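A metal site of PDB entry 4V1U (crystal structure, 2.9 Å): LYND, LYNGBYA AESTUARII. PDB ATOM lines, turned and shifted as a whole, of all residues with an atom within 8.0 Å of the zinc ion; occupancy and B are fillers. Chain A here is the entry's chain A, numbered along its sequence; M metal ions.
The side-chain sulfur (SG) of Cys 203 lies close to the backbone NH (N) of Asp 205 (3.4 Å). SG of Cys 206 sits close to N of Arg 308, at 3.5 Å. SG of Cys 311 sits close to N of Thr 313.
Within 4 Å of the zinc ion: Cys 203, Cys 206, Cys 311 and Cys 314. Along chain A the residues within 4 Å of the zinc ion span positions 203 to 314. The nearest printed residue that does not touch the zinc ion is Asp 205 (4.5 Å).
The zinc ion is bound by SG of Cys 203 (2.1 Å), SG of Cys 314 (2.1 Å), SG of Cys 206 (2.1 Å) and SG of Cys 311 (2.2 Å).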
ATOM      1  N   ASN A 170       3.576  14.705  13.531  1.00  0.00           N
ATOM      2  CA  ASN A 170       2.667  13.574  13.426  1.00  0.00           C
ATOM      3  C   ASN A 170       1.770  13.434  14.649  1.00  0.00           C
ATOM      4  O   ASN A 170       0.598  13.111  14.516  1.00  0.00           O
ATOM      5  CB  ASN A 170       3.459  12.283  13.239  1.00  0.00           C
ATOM      6  CG  ASN A 170       2.562  11.071  13.062  1.00  0.00           C
ATOM      7  OD1 ASN A 170       1.716  11.043  12.174  1.00  0.00           O
ATOM      8  ND2 ASN A 170       2.757  10.050  13.902  1.00  0.00           N
ATOM      9  N   LEU A 174      -2.504  13.741  15.152  1.00  0.00           N
ATOM     10  CA  LEU A 174      -3.318  12.688  15.739  1.00  0.00           C
ATOM     11  C   LEU A 174      -4.181  13.218  16.883  1.00  0.00           C
ATOM     12  O   LEU A 174      -5.317  12.791  17.072  1.00  0.00           O
ATOM     13  CB  LEU A 174      -2.431  11.549  16.244  1.00  0.00           C
ATOM     14  CG  LEU A 174      -1.658  10.793  15.163  1.00  0.00           C
ATOM     15  CD1 LEU A 174      -0.595   9.914  15.781  1.00  0.00           C
ATOM     16  CD2 LEU A 174      -2.581   9.966  14.284  1.00  0.00           C
ATOM     17  N   PHE A 196      -2.156  11.490   5.285  1.00  0.00           N
ATOM     18  CA  PHE A 196      -2.515  10.838   6.535  1.00  0.00           C
ATOM     19  C   PHE A 196      -3.883  11.312   7.000  1.00  0.00           C
ATOM     20  O   PHE A 196      -4.140  12.504   7.060  1.00  0.00           O
ATOM     21  CB  PHE A 196      -1.465  11.142   7.600  1.00  0.00           C
ATOM     22  CG  PHE A 196      -0.065  10.793   7.179  1.00  0.00           C
ATOM     23  CD1 PHE A 196       0.427   9.511   7.344  1.00  0.00           C
ATOM     24  CD2 PHE A 196       0.766  11.752   6.618  1.00  0.00           C
ATOM     25  CE1 PHE A 196       1.698   9.182   6.961  1.00  0.00           C
ATOM     26  CE2 PHE A 196       2.052  11.428   6.228  1.00  0.00           C
ATOM     27  CZ  PHE A 196       2.520  10.142   6.395  1.00  0.00           C
ATOM     28  N   THR A 201      -6.138   6.078   8.110  1.00  0.00           N
ATOM     29  CA  THR A 201      -4.889   5.627   7.505  1.00  0.00           C
ATOM     30  C   THR A 201      -3.796   5.463   8.541  1.00  0.00           C
ATOM     31  O   THR A 201      -3.983   5.770   9.707  1.00  0.00           O
ATOM     32  CB  THR A 201      -4.367   6.610   6.442  1.00  0.00           C
ATOM     33  OG1 THR A 201      -4.082   7.877   7.066  1.00  0.00           O
ATOM     34  CG2 THR A 201      -5.376   6.792   5.335  1.00  0.00           C
ATOM     35  N   GLY A 202      -2.642   4.984   8.094  1.00  0.00           N
ATOM     36  CA  GLY A 202      -1.481   4.886   8.970  1.00  0.00           C
ATOM     37  C   GLY A 202      -1.018   6.267   9.388  1.00  0.00           C
ATOM     38  O   GLY A 202      -1.351   7.258   8.747  1.00  0.00           O
ATOM     39  N   CYS A 203      -0.287   6.336  10.497  1.00  0.00           N
ATOM     40  CA  CYS A 203       0.343   7.576  10.898  1.00  0.00           C
ATOM     41  C   CYS A 203       1.700   7.630  10.218  1.00  0.00           C
ATOM     42  O   CYS A 203       2.058   6.723   9.487  1.00  0.00           O
ATOM     43  CB  CYS A 203       0.472   7.661  12.424  1.00  0.00           C
ATOM     44  SG  CYS A 203       1.533   6.398  13.173  1.00  0.00           S
ATOM     45  N   TRP A 204       2.432   8.723  10.437  1.00  0.00           N
ATOM     46  CA  TRP A 204       3.788   8.833   9.933  1.00  0.00           C
ATOM     47  C   TRP A 204       4.677   7.740  10.516  1.00  0.00           C
ATOM     48  O   TRP A 204       5.582   7.238   9.838  1.00  0.00           O
ATOM     49  CB  TRP A 204       4.387  10.184  10.274  1.00  0.00           C
ATOM     50  CG  TRP A 204       5.843  10.253   9.964  1.00  0.00           C
ATOM     51  CD1 TRP A 204       6.409  10.525   8.767  1.00  0.00           C
ATOM     52  CD2 TRP A 204       6.911  10.028  10.872  1.00  0.00           C
ATOM     53  NE1 TRP A 204       7.771  10.491   8.881  1.00  0.00           N
ATOM     54  CE2 TRP A 204       8.108  10.179  10.157  1.00  0.00           C
ATOM     55  CE3 TRP A 204       6.975   9.699  12.236  1.00  0.00           C
ATOM     56  CZ2 TRP A 204       9.359  10.046  10.753  1.00  0.00           C
ATOM     57  CZ3 TRP A 204       8.217   9.567  12.827  1.00  0.00           C
ATOM     58  CH2 TRP A 204       9.385   9.731  12.085  1.00  0.00           C
ATOM     59  N   ASP A 205       4.428   7.375  11.772  1.00  0.00           N
ATOM     60  CA  ASP A 205       5.224   6.390  12.462  1.00  0.00           C
ATOM     61  C   ASP A 205       4.955   4.988  11.921  1.00  0.00           C
ATOM     62  O   ASP A 205       5.877   4.171  11.805  1.00  0.00           O
ATOM     63  CB  ASP A 205       4.938   6.442  13.970  1.00  0.00           C
ATOM     64  CG  ASP A 205       6.020   5.767  14.796  1.00  0.00           C
ATOM     65  OD1 ASP A 205       7.061   5.369  14.239  1.00  0.00           O
ATOM     66  OD2 ASP A 205       5.805   5.639  16.016  1.00  0.00           O
ATOM     67  N   CYS A 206       3.694   4.710  11.573  1.00  0.00           N
ATOM     68  CA  CYS A 206       3.364   3.463  10.888  1.00  0.00           C
ATOM     69  C   CYS A 206       4.193   3.336   9.603  1.00  0.00           C
ATOM     70  O   CYS A 206       4.668   2.264   9.261  1.00  0.00           O
ATOM     71  CB  CYS A 206       1.867   3.415  10.544  1.00  0.00           C
ATOM     72  SG  CYS A 206       0.775   3.130  11.953  1.00  0.00           S
ATOM     73  N   LEU A 207       4.383   4.455   8.907  1.00  0.00           N
ATOM     74  CA  LEU A 207       5.244   4.508   7.728  1.00  0.00           C
ATOM     75  C   LEU A 207       6.728   4.469   8.093  1.00  0.00           C
ATOM     76  O   LEU A 207       7.520   3.764   7.461  1.00  0.00           O
ATOM     77  CB  LEU A 207       4.966   5.780   6.932  1.00  0.00           C
ATOM     78  CG  LEU A 207       5.983   6.138   5.855  1.00  0.00           C
ATOM     79  CD1 LEU A 207       5.980   5.114   4.746  1.00  0.00           C
ATOM     80  CD2 LEU A 207       5.701   7.507   5.278  1.00  0.00           C
ATOM     81  N   ALA A 208       7.109   5.259   9.092  1.00  0.00           N
ATOM     82  CA  ALA A 208       8.510   5.381   9.471  1.00  0.00           C
ATOM     83  C   ALA A 208       9.083   4.063   9.936  1.00  0.00           C
ATOM     84  O   ALA A 208      10.287   3.821   9.803  1.00  0.00           O
ATOM     85  CB  ALA A 208       8.670   6.443  10.548  1.00  0.00           C
ATOM     86  N   HIS A 209       8.235   3.202  10.493  1.00  0.00           N
ATOM     87  CA  HIS A 209       8.685   1.890  10.934  1.00  0.00           C
ATOM     88  C   HIS A 209       9.192   1.067   9.754  1.00  0.00           C
ATOM     89  O   HIS A 209      10.147   0.311   9.886  1.00  0.00           O
ATOM     90  CB  HIS A 209       7.547   1.142  11.633  1.00  0.00           C
ATOM     91  CG  HIS A 209       7.951  -0.185  12.206  1.00  0.00           C
ATOM     92  ND1 HIS A 209       7.928  -1.351  11.475  1.00  0.00           N
ATOM     93  CD2 HIS A 209       8.394  -0.520  13.447  1.00  0.00           C
ATOM     94  CE1 HIS A 209       8.326  -2.358  12.231  1.00  0.00           C
ATOM     95  NE2 HIS A 209       8.614  -1.873  13.431  1.00  0.00           N
ATOM     96  N   LEU A 305       0.504   2.368   1.901  1.00  0.00           N
ATOM     97  CA  LEU A 305       0.800   2.423   3.330  1.00  0.00           C
ATOM     98  C   LEU A 305      -0.255   1.659   4.106  1.00  0.00           C
ATOM     99  O   LEU A 305      -1.448   1.916   3.954  1.00  0.00           O
ATOM    100  CB  LEU A 305       0.862   3.877   3.807  1.00  0.00           C
ATOM    101  CG  LEU A 305       1.042   4.092   5.316  1.00  0.00           C
ATOM    102  CD1 LEU A 305       2.410   3.585   5.762  1.00  0.00           C
ATOM    103  CD2 LEU A 305       0.853   5.558   5.687  1.00  0.00           C
ATOM    104  N   ILE A 306       0.185   0.729   4.937  1.00  0.00           N
ATOM    105  CA  ILE A 306      -0.714  -0.036   5.807  1.00  0.00           C
ATOM    106  C   ILE A 306      -0.739   0.527   7.206  1.00  0.00           C
ATOM    107  O   ILE A 306       0.314   0.810   7.788  1.00  0.00           O
ATOM    108  CB  ILE A 306      -0.288  -1.525   5.904  1.00  0.00           C
ATOM    109  CG1 ILE A 306      -0.312  -2.186   4.524  1.00  0.00           C
ATOM    110  CG2 ILE A 306      -1.193  -2.294   6.852  1.00  0.00           C
ATOM    111  CD1 ILE A 306       1.060  -2.341   3.927  1.00  0.00           C
ATOM    112  N   LYS A 307      -1.935   0.682   7.769  1.00  0.00           N
ATOM    113  CA  LYS A 307      -2.066   1.140   9.141  1.00  0.00           C
ATOM    114  C   LYS A 307      -1.763  -0.016  10.083  1.00  0.00           C
ATOM    115  O   LYS A 307      -2.443  -1.028  10.079  1.00  0.00           O
ATOM    116  CB  LYS A 307      -3.480   1.661   9.400  1.00  0.00           C
ATOM    117  CG  LYS A 307      -3.655   2.307  10.763  1.00  0.00           C
ATOM    118  CD  LYS A 307      -5.116   2.577  11.078  1.00  0.00           C
ATOM    119  CE  LYS A 307      -5.300   2.972  12.538  1.00  0.00           C
ATOM    120  NZ  LYS A 307      -6.726   3.179  12.900  1.00  0.00           N
ATOM    121  N   ARG A 308      -0.732   0.150  10.897  1.00  0.00           N
ATOM    122  CA  ARG A 308      -0.307  -0.907  11.807  1.00  0.00           C
ATOM    123  C   ARG A 308      -1.179  -0.892  13.051  1.00  0.00           C
ATOM    124  O   ARG A 308      -1.262   0.132  13.722  1.00  0.00           O
ATOM    125  CB  ARG A 308       1.160  -0.740  12.180  1.00  0.00           C
ATOM    126  CG  ARG A 308       2.106  -0.753  10.992  1.00  0.00           C
ATOM    127  CD  ARG A 308       3.547  -0.523  11.436  1.00  0.00           C
ATOM    128  NE  ARG A 308       4.204  -1.748  11.898  1.00  0.00           N
ATOM    129  CZ  ARG A 308       4.841  -1.885  13.062  1.00  0.00           C
ATOM    130  NH1 ARG A 308       4.926  -0.887  13.931  1.00  0.00           N
ATOM    131  NH2 ARG A 308       5.400  -3.044  13.357  1.00  0.00           N
ATOM    132  N   SER A 309      -1.815  -2.014  13.352  1.00  0.00           N
ATOM    133  CA  SER A 309      -2.664  -2.111  14.538  1.00  0.00           C
ATOM    134  C   SER A 309      -1.823  -1.918  15.783  1.00  0.00           C
ATOM    135  O   SER A 309      -2.263  -1.291  16.746  1.00  0.00           O
ATOM    136  CB  SER A 309      -3.361  -3.472  14.612  1.00  0.00           C
ATOM    137  OG  SER A 309      -3.896  -3.842  13.355  1.00  0.00           O
ATOM    138  N   GLN A 310      -0.607  -2.469  15.752  1.00  0.00           N
ATOM    139  CA  GLN A 310       0.273  -2.449  16.909  1.00  0.00           C
ATOM    140  C   GLN A 310       1.108  -1.175  17.004  1.00  0.00           C
ATOM    141  O   GLN A 310       1.964  -1.057  17.880  1.00  0.00           O
ATOM    142  CB  GLN A 310       1.206  -3.671  16.890  1.00  0.00           C
ATOM    143  CG  GLN A 310       2.319  -3.622  15.861  1.00  0.00           C
ATOM    144  CD  GLN A 310       1.990  -4.374  14.589  1.00  0.00           C
ATOM    145  OE1 GLN A 310       0.856  -4.342  14.111  1.00  0.00           O
ATOM    146  NE2 GLN A 310       2.992  -5.053  14.044  1.00  0.00           N
ATOM    147  N   CYS A 311       0.871  -0.230  16.089  1.00  0.00           N
ATOM    148  CA  CYS A 311       1.629   1.012  16.080  1.00  0.00           C
ATOM    149  C   CYS A 311       1.636   1.664  17.443  1.00  0.00           C
ATOM    150  O   CYS A 311       0.573   1.891  18.010  1.00  0.00           O
ATOM    151  CB  CYS A 311       1.073   1.988  15.068  1.00  0.00           C
ATOM    152  SG  CYS A 311       1.991   3.552  15.088  1.00  0.00           S
ATOM    153  N   PRO A 312       2.827   1.948  17.997  1.00  0.00           N
ATOM    154  CA  PRO A 312       2.853   2.617  19.306  1.00  0.00           C
ATOM    155  C   PRO A 312       2.152   3.969  19.332  1.00  0.00           C
ATOM    156  O   PRO A 312       1.553   4.320  20.344  1.00  0.00           O
ATOM    157  CB  PRO A 312       4.359   2.790  19.603  1.00  0.00           C
ATOM    158  CG  PRO A 312       5.063   2.534  18.302  1.00  0.00           C
ATOM    159  CD  PRO A 312       4.180   1.611  17.516  1.00  0.00           C
ATOM    160  N   THR A 313       2.192   4.711  18.229  1.00  0.00           N
ATOM    161  CA  THR A 313       1.722   6.083  18.229  1.00  0.00           C
ATOM    162  C   THR A 313       0.214   6.230  18.014  1.00  0.00           C
ATOM    163  O   THR A 313      -0.408   7.039  18.701  1.00  0.00           O
ATOM    164  CB  THR A 313       2.436   6.894  17.135  1.00  0.00           C
ATOM    165  OG1 THR A 313       3.856   6.749  17.299  1.00  0.00           O
ATOM    166  CG2 THR A 313       2.054   8.358  17.237  1.00  0.00           C
ATOM    167  N   CYS A 314      -0.360   5.481  17.074  1.00  0.00           N
ATOM    168  CA  CYS A 314      -1.810   5.564  16.768  1.00  0.00           C
ATOM    169  C   CYS A 314      -2.609   4.295  17.076  1.00  0.00           C
ATOM    170  O   CYS A 314      -3.833   4.290  16.991  1.00  0.00           O
ATOM    171  CB  CYS A 314      -2.022   5.962  15.293  1.00  0.00           C
ATOM    172  SG  CYS A 314      -1.251   4.890  14.047  1.00  0.00           S
ATOM    173  N   GLY A 315      -1.917   3.223  17.449  1.00  0.00           N
ATOM    174  CA  GLY A 315      -2.552   1.941  17.743  1.00  0.00           C
ATOM    175  C   GLY A 315      -2.238   1.472  19.150  1.00  0.00           C
ATOM    176  O   GLY A 315      -1.956   2.282  20.017  1.00  0.00           O
ATOM    177  N   ASP A 316      -2.264   0.150  19.344  1.00  0.00           N
ATOM    178  CA  ASP A 316      -1.998  -0.475  20.640  1.00  0.00           C
ATOM    179  C   ASP A 316      -0.772  -1.367  20.548  1.00  0.00           C
ATOM    180  O   ASP A 316      -0.822  -2.420  19.930  1.00  0.00           O
ATOM    181  CB  ASP A 316      -3.216  -1.304  21.088  1.00  0.00           C
ATOM    182  CG  ASP A 316      -2.972  -2.071  22.384  1.00  0.00           C
ATOM    183  OD1 ASP A 316      -2.169  -1.621  23.224  1.00  0.00           O
ATOM    184  OD2 ASP A 316      -3.600  -3.126  22.554  1.00  0.00           O
HETATM  185 ZN    ZN M   1       0.743   4.536  13.520  1.00  0.00          ZN
